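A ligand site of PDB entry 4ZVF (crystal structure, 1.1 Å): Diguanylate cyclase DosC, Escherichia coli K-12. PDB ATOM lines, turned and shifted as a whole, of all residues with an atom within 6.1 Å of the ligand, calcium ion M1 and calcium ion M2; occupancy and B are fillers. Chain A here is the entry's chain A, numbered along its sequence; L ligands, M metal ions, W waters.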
ATOM      1  N   ASP A  37      16.533  21.829  32.119  1.00  0.00           N
ATOM      2  CA  ASP A  37      15.941  21.436  30.855  1.00  0.00           C
ATOM      3  C   ASP A  37      17.050  21.324  29.817  1.00  0.00           C
ATOM      4  O   ASP A  37      17.797  22.275  29.570  1.00  0.00           O
ATOM      5  CB  ASP A  37      14.896  22.493  30.484  1.00  0.00           C
ATOM      6  CG  ASP A  37      14.164  22.196  29.210  1.00  0.00           C
ATOM      7  OD1 ASP A  37      14.821  21.921  28.198  1.00  0.00           O
ATOM      8  OD2 ASP A  37      12.920  22.309  29.199  1.00  0.00           O
ATOM      9  N   VAL A  38      17.181  20.140  29.209  1.00  0.00           N
ATOM     10  CA  VAL A  38      18.251  19.903  28.246  1.00  0.00           C
ATOM     11  C   VAL A  38      18.072  20.786  27.021  1.00  0.00           C
ATOM     12  O   VAL A  38      16.958  20.931  26.500  1.00  0.00           O
ATOM     13  CB  VAL A  38      18.328  18.416  27.820  1.00  0.00           C
ATOM     14  CG1 VAL A  38      19.471  18.184  26.815  1.00  0.00           C
ATOM     15  CG2 VAL A  38      18.489  17.529  29.061  1.00  0.00           C
ATOM     16  N   ASP A  39      19.164  21.377  26.548  1.00  0.00           N
ATOM     17  CA  ASP A  39      19.123  22.293  25.414  1.00  0.00           C
ATOM     18  C   ASP A  39      19.041  21.561  24.088  1.00  0.00           C
ATOM     19  O   ASP A  39      19.825  20.631  23.821  1.00  0.00           O
ATOM     20  CB  ASP A  39      20.363  23.175  25.419  1.00  0.00           C
ATOM     21  CG  ASP A  39      20.376  24.180  26.560  1.00  0.00           C
ATOM     22  OD1 ASP A  39      19.298  24.566  27.055  1.00  0.00           O
ATOM     23  OD2 ASP A  39      21.486  24.582  26.941  1.00  0.00           O
ATOM     24  N   LYS A  40      18.079  21.952  23.263  1.00  0.00           N
ATOM     25  CA  LYS A  40      17.998  21.478  21.858  1.00  0.00           C
ATOM     26  C   LYS A  40      18.046  19.945  21.796  1.00  0.00           C
ATOM     27  O   LYS A  40      18.733  19.346  20.962  1.00  0.00           O
ATOM     28  CB  LYS A  40      19.095  22.115  20.993  1.00  0.00           C
ATOM     29  CG  LYS A  40      18.992  23.638  20.945  1.00  0.00           C
ATOM     30  CD  LYS A  40      19.930  24.272  19.917  1.00  0.00           C
ATOM     31  CE  LYS A  40      19.791  25.798  19.879  1.00  0.00           C
ATOM     32  NZ  LYS A  40      20.634  26.404  18.803  1.00  0.00           N
ATOM     33  N   PHE A  41      17.300  19.326  22.702  1.00  0.00           N
ATOM     34  CA  PHE A  41      17.269  17.873  22.797  1.00  0.00           C
ATOM     35  C   PHE A  41      16.631  17.231  21.555  1.00  0.00           C
ATOM     36  O   PHE A  41      16.987  16.110  21.177  1.00  0.00           O
ATOM     37  CB  PHE A  41      16.540  17.457  24.077  1.00  0.00           C
ATOM     38  CG  PHE A  41      16.790  16.034  24.495  1.00  0.00           C
ATOM     39  CD1 PHE A  41      18.078  15.520  24.560  1.00  0.00           C
ATOM     40  CD2 PHE A  41      15.732  15.229  24.864  1.00  0.00           C
ATOM     41  CE1 PHE A  41      18.295  14.206  24.968  1.00  0.00           C
ATOM     42  CE2 PHE A  41      15.943  13.917  25.291  1.00  0.00           C
ATOM     43  CZ  PHE A  41      17.222  13.417  25.330  1.00  0.00           C
ATOM     44  N   LYS A  42      15.701  17.928  20.909  1.00  0.00           N
ATOM     45  CA  LYS A  42      15.143  17.427  19.656  1.00  0.00           C
ATOM     46  C   LYS A  42      16.244  17.285  18.608  1.00  0.00           C
ATOM     47  O   LYS A  42      16.325  16.271  17.905  1.00  0.00           O
ATOM     48  CB  LYS A  42      14.016  18.314  19.140  1.00  0.00           C
ATOM     49  CG  LYS A  42      13.432  17.855  17.812  1.00  0.00           C
ATOM     50  CD  LYS A  42      12.333  18.773  17.313  1.00  0.00           C
ATOM     51  CE  LYS A  42      11.054  18.590  18.129  1.00  0.00           C
ATOM     52  NZ  LYS A  42       9.853  19.080  17.390  1.00  0.00           N
ATOM     53  N   GLU A  43      17.113  18.286  18.519  1.00  0.00           N
ATOM     54  CA  GLU A  43      18.238  18.230  17.596  1.00  0.00           C
ATOM     55  C   GLU A  43      19.210  17.115  17.951  1.00  0.00           C
ATOM     56  O   GLU A  43      19.745  16.446  17.057  1.00  0.00           O
ATOM     57  CB  GLU A  43      18.976  19.577  17.548  1.00  0.00           C
ATOM     58  CG  GLU A  43      18.192  20.701  16.882  1.00  0.00           C
ATOM     59  CD  GLU A  43      19.004  21.969  16.697  1.00  0.00           C
ATOM     60  OE1 GLU A  43      18.423  23.003  16.290  1.00  0.00           O
ATOM     61  OE2 GLU A  43      20.231  21.945  16.956  1.00  0.00           O
ATOM     62  N   ASN A  45      18.453  14.240  19.417  1.00  0.00           N
ATOM     63  CA  ASN A  45      17.819  12.999  18.981  1.00  0.00           C
ATOM     64  C   ASN A  45      17.786  12.849  17.464  1.00  0.00           C
ATOM     65  O   ASN A  45      17.977  11.759  16.949  1.00  0.00           O
ATOM     66  CB  ASN A  45      16.410  12.877  19.553  1.00  0.00           C
ATOM     67  CG  ASN A  45      16.406  12.507  21.027  1.00  0.00           C
ATOM     68  OD1 ASN A  45      16.674  11.367  21.381  1.00  0.00           O
ATOM     69  ND2 ASN A  45      16.106  13.462  21.879  1.00  0.00           N
ATOM     70  N   GLY A  49      20.357  10.087  17.231  1.00  0.00           N
ATOM     71  CA  GLY A  49      19.452   8.981  17.508  1.00  0.00           C
ATOM     72  C   GLY A  49      18.841   8.977  18.898  1.00  0.00           C
ATOM     73  O   GLY A  49      19.400   9.536  19.851  1.00  0.00           O
ATOM     74  N   HIS A  50      17.668   8.346  19.004  1.00  0.00           N
ATOM     75  CA  HIS A  50      16.920   8.268  20.255  1.00  0.00           C
ATOM     76  C   HIS A  50      17.720   7.550  21.357  1.00  0.00           C
ATOM     77  O   HIS A  50      17.665   7.950  22.518  1.00  0.00           O
ATOM     78  CB  HIS A  50      15.592   7.551  19.997  1.00  0.00           C
ATOM     79  CG  HIS A  50      14.595   7.652  21.123  1.00  0.00           C
ATOM     80  ND1 HIS A  50      14.596   6.794  22.207  1.00  0.00           N
ATOM     81  CD2 HIS A  50      13.559   8.496  21.311  1.00  0.00           C
ATOM     82  CE1 HIS A  50      13.611   7.120  23.019  1.00  0.00           C
ATOM     83  NE2 HIS A  50      12.962   8.148  22.509  1.00  0.00           N
ATOM     84  N   ASN A  51      18.444   6.494  20.991  1.00  0.00           N
ATOM     85  CA  ASN A  51      19.279   5.774  21.957  1.00  0.00           C
ATOM     86  C   ASN A  51      20.363   6.675  22.542  1.00  0.00           C
ATOM     87  O   ASN A  51      20.619   6.660  23.745  1.00  0.00           O
ATOM     88  CB  ASN A  51      19.904   4.503  21.350  1.00  0.00           C
ATOM     89  CG  ASN A  51      18.902   3.352  21.204  1.00  0.00           C
ATOM     90  OD1 ASN A  51      18.358   3.110  20.129  1.00  0.00           O
ATOM     91  ND2 ASN A  51      18.671   2.624  22.288  1.00  0.00           N
ATOM     92  N   THR A  52      21.003   7.472  21.680  1.00  0.00           N
ATOM     93  CA  THR A  52      22.004   8.426  22.171  1.00  0.00           C
ATOM     94  C   THR A  52      21.354   9.436  23.121  1.00  0.00           C
ATOM     95  O   THR A  52      21.911   9.769  24.192  1.00  0.00           O
ATOM     96  CB  THR A  52      22.726   9.153  21.026  1.00  0.00           C
ATOM     97  OG1 THR A  52      23.348   8.174  20.190  1.00  0.00           O
ATOM     98  CG2 THR A  52      23.783  10.075  21.611  1.00  0.00           C
ATOM     99  N   GLY A  53      20.158   9.898  22.764  1.00  0.00           N
ATOM    100  CA  GLY A  53      19.405  10.798  23.632  1.00  0.00           C
ATOM    101  C   GLY A  53      19.165  10.187  25.006  1.00  0.00           C
ATOM    102  O   GLY A  53      19.337  10.857  26.031  1.00  0.00           O
ATOM    103  N   ASP A  54      18.816   8.908  25.039  1.00  0.00           N
ATOM    104  CA  ASP A  54      18.582   8.210  26.298  1.00  0.00           C
ATOM    105  C   ASP A  54      19.875   8.101  27.122  1.00  0.00           C
ATOM    106  O   ASP A  54      19.837   8.217  28.348  1.00  0.00           O
ATOM    107  CB  ASP A  54      17.984   6.825  26.057  1.00  0.00           C
ATOM    108  CG  ASP A  54      16.483   6.866  25.733  1.00  0.00           C
ATOM    109  OD1 ASP A  54      15.909   7.958  25.596  1.00  0.00           O
ATOM    110  OD2 ASP A  54      15.879   5.770  25.597  1.00  0.00           O
ATOM    111  N   LEU A  57      20.467  11.435  28.751  1.00  0.00           N
ATOM    112  CA  LEU A  57      19.644  11.620  29.953  1.00  0.00           C
ATOM    113  C   LEU A  57      20.295  10.987  31.190  1.00  0.00           C
ATOM    114  O   LEU A  57      20.218  11.557  32.275  1.00  0.00           O
ATOM    115  CB  LEU A  57      18.223  11.086  29.743  1.00  0.00           C
ATOM    116  CG  LEU A  57      17.382  11.872  28.737  1.00  0.00           C
ATOM    117  CD1 LEU A  57      16.058  11.175  28.426  1.00  0.00           C
ATOM    118  CD2 LEU A  57      17.152  13.319  29.172  1.00  0.00           C
ATOM    119  N   ARG A  76      12.654  13.409  38.234  1.00  0.00           N
ATOM    120  CA  ARG A  76      12.343  13.448  36.823  1.00  0.00           C
ATOM    121  C   ARG A  76      11.024  14.199  36.651  1.00  0.00           C
ATOM    122  O   ARG A  76       9.998  13.774  37.181  1.00  0.00           O
ATOM    123  CB  ARG A  76      12.166  12.026  36.293  1.00  0.00           C
ATOM    124  CG  ARG A  76      11.910  11.927  34.797  1.00  0.00           C
ATOM    125  CD  ARG A  76      13.195  12.141  34.000  1.00  0.00           C
ATOM    126  NE  ARG A  76      12.992  12.022  32.554  1.00  0.00           N
ATOM    127  CZ  ARG A  76      13.141  10.897  31.862  1.00  0.00           C
ATOM    128  NH1 ARG A  76      13.493   9.775  32.481  1.00  0.00           N
ATOM    129  NH2 ARG A  76      12.939  10.893  30.541  1.00  0.00           N
ATOM    130  N   GLY A  78       9.910  15.777  33.446  1.00  0.00           N
ATOM    131  CA  GLY A  78       9.366  15.624  32.110  1.00  0.00           C
ATOM    132  C   GLY A  78      10.348  14.830  31.280  1.00  0.00           C
ATOM    133  O   GLY A  78      11.342  14.345  31.809  1.00  0.00           O
ATOM    134  N   GLY A  79      10.088  14.741  29.971  1.00  0.00           N
ATOM    135  CA  GLY A  79      10.960  14.000  29.061  1.00  0.00           C
ATOM    136  C   GLY A  79      12.429  14.357  29.198  1.00  0.00           C
ATOM    137  O   GLY A  79      13.288  13.480  29.295  1.00  0.00           O
ATOM    138  N   ASP A  80      12.725  15.656  29.210  1.00  0.00           N
ATOM    139  CA  ASP A  80      14.102  16.122  29.340  1.00  0.00           C
ATOM    140  C   ASP A  80      14.193  17.249  30.356  1.00  0.00           C
ATOM    141  O   ASP A  80      15.031  18.144  30.238  1.00  0.00           O
ATOM    142  CB  ASP A  80      14.687  16.561  27.982  1.00  0.00           C
ATOM    143  CG  ASP A  80      14.063  17.837  27.444  1.00  0.00           C
ATOM    144  OD1 ASP A  80      12.860  18.070  27.675  1.00  0.00           O
ATOM    145  OD2 ASP A  80      14.794  18.597  26.771  1.00  0.00           O
ATOM    146  N   GLU A  81      13.321  17.156  31.361  1.00  0.00           N
ATOM    147  CA  GLU A  81      13.221  18.162  32.405  1.00  0.00           C
ATOM    148  C   GLU A  81      13.329  17.517  33.773  1.00  0.00           C
ATOM    149  O   GLU A  81      12.833  16.408  33.997  1.00  0.00           O
ATOM    150  CB  GLU A  81      11.893  18.905  32.316  1.00  0.00           C
ATOM    151  CG  GLU A  81      11.805  19.860  31.133  1.00  0.00           C
ATOM    152  CD  GLU A  81      10.878  19.367  30.050  1.00  0.00           C
ATOM    153  OE1 GLU A  81      10.341  18.242  30.179  1.00  0.00           O
ATOM    154  OE2 GLU A  81      10.687  20.112  29.067  1.00  0.00           O
ATOM    155  N   LEU A 146      13.834  29.836  34.095  1.00  0.00           N
ATOM    156  CA  LEU A 146      14.308  28.871  33.087  1.00  0.00           C
ATOM    157  C   LEU A 146      14.005  29.376  31.674  1.00  0.00           C
ATOM    158  O   LEU A 146      14.848  29.297  30.762  1.00  0.00           O
ATOM    159  CB  LEU A 146      13.652  27.512  33.307  1.00  0.00           C
ATOM    160  CG  LEU A 146      13.946  26.466  32.242  1.00  0.00           C
ATOM    161  CD1 LEU A 146      15.449  26.194  32.106  1.00  0.00           C
ATOM    162  CD2 LEU A 146      13.176  25.180  32.547  1.00  0.00           C
ATOM    163  N   LYS A 150      16.646  30.212  28.612  1.00  0.00           N
ATOM    164  CA  LYS A 150      16.501  29.718  27.242  1.00  0.00           C
ATOM    165  C   LYS A 150      16.501  30.873  26.254  1.00  0.00           C
ATOM    166  O   LYS A 150      17.223  30.862  25.246  1.00  0.00           O
ATOM    167  CB  LYS A 150      15.206  28.912  27.087  1.00  0.00           C
ATOM    168  CG  LYS A 150      15.156  27.576  27.826  1.00  0.00           C
ATOM    169  CD  LYS A 150      16.022  26.492  27.179  1.00  0.00           C
ATOM    170  CE  LYS A 150      15.678  25.119  27.749  1.00  0.00           C
ATOM    171  NZ  LYS A 150      16.533  24.027  27.194  1.00  0.00           N
ATOM    172  N   ARG A 154      20.408  29.919  25.983  1.00  0.00           N
ATOM    173  CA  ARG A 154      20.635  28.557  26.504  1.00  0.00           C
ATOM    174  C   ARG A 154      22.045  28.407  27.073  1.00  0.00           C
ATOM    175  O   ARG A 154      22.816  29.368  27.126  1.00  0.00           O
ATOM    176  CB  ARG A 154      20.333  27.488  25.449  1.00  0.00           C
ATOM    177  CG  ARG A 154      18.925  27.551  24.910  1.00  0.00           C
ATOM    178  CD  ARG A 154      18.713  26.448  23.885  1.00  0.00           C
ATOM    179  NE  ARG A 154      17.320  26.333  23.432  1.00  0.00           N
ATOM    180  CZ  ARG A 154      16.800  27.010  22.418  1.00  0.00           C
ATOM    181  NH1 ARG A 154      15.528  26.807  22.074  1.00  0.00           N
ATOM    182  NH2 ARG A 154      17.525  27.901  21.741  1.00  0.00           N
HETATM  183  O1  LIG L   1      12.677   9.838  27.219  1.00  0.00           O
HETATM  184  C1  LIG L   1      13.077  10.438  26.219  1.00  0.00           C
HETATM  185  C2  LIG L   1      12.406  11.688  25.754  1.00  0.00           C
HETATM  186  C3  LIG L   1      12.850  12.347  24.657  1.00  0.00           C
HETATM  187  N1  LIG L   1      13.989  11.835  23.910  1.00  0.00           N
HETATM  188  C4  LIG L   1      14.617  10.634  24.357  1.00  0.00           C
HETATM  189  N2  LIG L   1      15.718  10.125  23.661  1.00  0.00           N
HETATM  190  N3  LIG L   1      14.169   9.954  25.508  1.00  0.00           N
HETATM  191  N4  LIG L   1      11.363  12.349  26.252  1.00  0.00           N
HETATM  192  C5  LIG L   1      11.152  13.430  25.471  1.00  0.00           C
HETATM  193  N5  LIG L   1      12.055  13.415  24.486  1.00  0.00           N
HETATM  194  C6  LIG L   1      12.449  14.211  23.361  1.00  0.00           C
HETATM  195  C7  LIG L   1      11.168  14.615  22.564  1.00  0.00           C
HETATM  196  O2  LIG L   1      10.874  13.680  21.602  1.00  0.00           O
HETATM  197  C8  LIG L   1      11.514  15.977  22.007  1.00  0.00           C
HETATM  198  O3  LIG L   1      11.914  15.835  20.578  1.00  0.00           O
HETATM  199  O4  LIG L   1      12.810  15.351  23.860  1.00  0.00           O
HETATM  200  C9  LIG L   1      12.539  16.438  22.734  1.00  0.00           C
HETATM  201  C10 LIG L   1      12.280  17.754  23.405  1.00  0.00           C
HETATM  202  O5  LIG L   1      12.218  18.709  22.345  1.00  0.00           O
HETATM  203  P1  LIG L   1      11.534  20.136  22.540  1.00  0.00           P
HETATM  204  S1  LIG L   1      10.111  20.115  24.021  1.00  0.00           S
HETATM  205  O6  LIG L   1      10.934  20.591  21.251  1.00  0.00           O
HETATM  206  O7  LIG L   1      12.664  21.139  23.002  1.00  0.00           O
HETATM  207  P2  LIG L   1      14.258  21.101  22.797  1.00  0.00           P
HETATM  208  O8  LIG L   1      14.941  20.404  23.936  1.00  0.00           O
HETATM  209  O9  LIG L   1      14.615  20.569  21.426  1.00  0.00           O
HETATM  210  O10 LIG L   1      14.619  22.674  22.854  1.00  0.00           O
HETATM  211  P3  LIG L   1      14.707  23.650  24.105  1.00  0.00           P
HETATM  212  O11 LIG L   1      16.196  23.870  24.325  1.00  0.00           O
HETATM  213  O12 LIG L   1      13.992  24.914  23.719  1.00  0.00           O
HETATM  214  O13 LIG L   1      14.088  22.926  25.281  1.00  0.00           O
HETATM  215 CA    CA M   1      14.655  20.824  26.190  1.00  0.00          CA
HETATM  216 CA    CA M   2      10.902  22.053  28.024  1.00  0.00          CA
HETATM  217  O   HOH W   1      12.242  20.407  26.549  1.00  0.00           O
HETATM  218  O   HOH W   2      11.706  23.430  26.271  1.00  0.00           O
HETATM  219  O   HOH W   3       8.736  21.903  27.003  1.00  0.00           O
HETATM  220  O   HOH W   4       8.829  23.057  20.910  1.00  0.00           O
HETATM  221  O   HOH W   5       9.997  23.610  29.535  1.00  0.00           O
HETATM  222  O   HOH W   6      16.037  21.102  19.232  1.00  0.00           O
HETATM  223  O   HOH W   7      11.475   7.132  26.821  1.00  0.00           O
HETATM  224  O   HOH W   8      11.571  24.927  28.358  1.00  0.00           O
HETATM  225  O   HOH W   9      12.308  22.459  19.559  1.00  0.00           O
HETATM  226  O   HOH W  10      12.729  26.572  25.342  1.00  0.00           O
HETATM  227  O   HOH W  11      13.405   7.976  29.664  1.00  0.00           O
HETATM  228  O   HOH W  12       9.035  11.236  27.631  1.00  0.00           O
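OD1 of Asp 54 lies within hydrogen-bond range of N3 of the ligand (2.6 Å). A nitrogen (N2) of the ligand sits at hydrogen-bond distance from the side-chain amide oxygen (OD1) of Asn 45. An oxygen (O11) of the ligand lies within salt-bridge range of the guanidinium group of Arg 154, 2.9 Å away. The backbone NH (N) of Phe 41 sits at hydrogen-bond distance from an oxygen (O9) of the ligand, at 3.2 Å. An oxygen (O11) of the ligand lies within hydrogen-bond range of the backbone NH of Lys 40. NZ of Lys 150 lies within salt-bridge range of O11 of the ligand (2.9 Å). N of Lys 42 sits at hydrogen-bond distance from O9 of the ligand. O of His 50 sits at hydrogen-bond distance from N2 of the ligand (3.1 Å). The guanidinium group of Arg 76 is in hydrogen-bond range of an oxygen (O1) of the ligand, 3.5 Å away.
The backbone carbonyl oxygen (O) of Asp 37 lies within hydrogen-bond range of the side-chain amino group (NZ) of Lys 150 (3.2 Å). The side-chain amino group of Lys 150 sits close to the backbone carbonyl oxygen of Val 38, at 3.2 Å. ND2 of Asn 45 is in hydrogen-bond range of O of Phe 41, at 2.9 Å. The side-chain amino group (NZ) of Lys 150 is in salt-bridge range of the side-chain carboxylate (OD1) of Asp 39. The guanidinium group of Arg 76 lies within hydrogen-bond range of the backbone carbonyl oxygen of Gly 79 (2.9 Å). NE of Arg 76 is in hydrogen-bond range of O of Gly 78, 2.9 Å away.
Asp 39 touches the ligand (CA to O11, 3.5 Å). C of Gly 53 touches N2 of the ligand (3.7 Å). Leu 57 touches the ligand (CD1 to N3, 3.7 Å). Gly 79 touches the ligand. Within 4 Å of the ligand: Asp 37, Val 38, Asp 39, Lys 40, Phe 41, Lys 42, Asn 45, His 50, Gly 53, Asp 54, Leu 57, Arg 76, Gly 79, Asp 80, Lys 150 and Arg 154.
Residues that only touch calcium ion M1: Lys 150 (3.8 Å). Within 4 Å of calcium ion M1: Asp 37, Val 38, Asp 80 and Lys 150.
Within 4 Å of calcium ion M2: Asp 37 and Glu 81. The nearest printed residue that does not touch calcium ion M2 is Asp 80 (4.5 Å).
Calcium ion M1 is bound by OD1 of Asp 37 (2.3 Å). OD2 of Asp 80 is bound to calcium ion M1, at 2.3 Å. Calcium ion M1 is bound by O8 of the ligand (2.3 Å). Calcium ion M1 is bound by O of Val 38 (2.3 Å). O13 of the ligand binds calcium ion M1 (2.4 Å). Water W1 is bound to calcium ion M1 (2.5 Å). Calcium ion M1 has six donor atoms within binding distance.
Calcium ion M2 is bound by OE2 of Glu 81 (2.2 Å), OD2 of Asp 37 (2.3 Å), water W5 (2.4 Å), water W2 (2.4 Å), water W3 (2.4 Å) and water W1 (2.6 Å). Slightly farther from calcium ion M2 lies water W8 (3.0 Å).
Water W1 lies within hydrogen-bond range of OD1 of Asp 80 (2.7 Å) and S1 of the ligand (3.3 Å). Water W6 lies within hydrogen-bond range of an oxygen (O9) of the ligand and the backbone NH of Glu 43. Water W11 lies within hydrogen-bond range of the guanidinium group of Arg 76 and an oxygen (O1) of the ligand.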
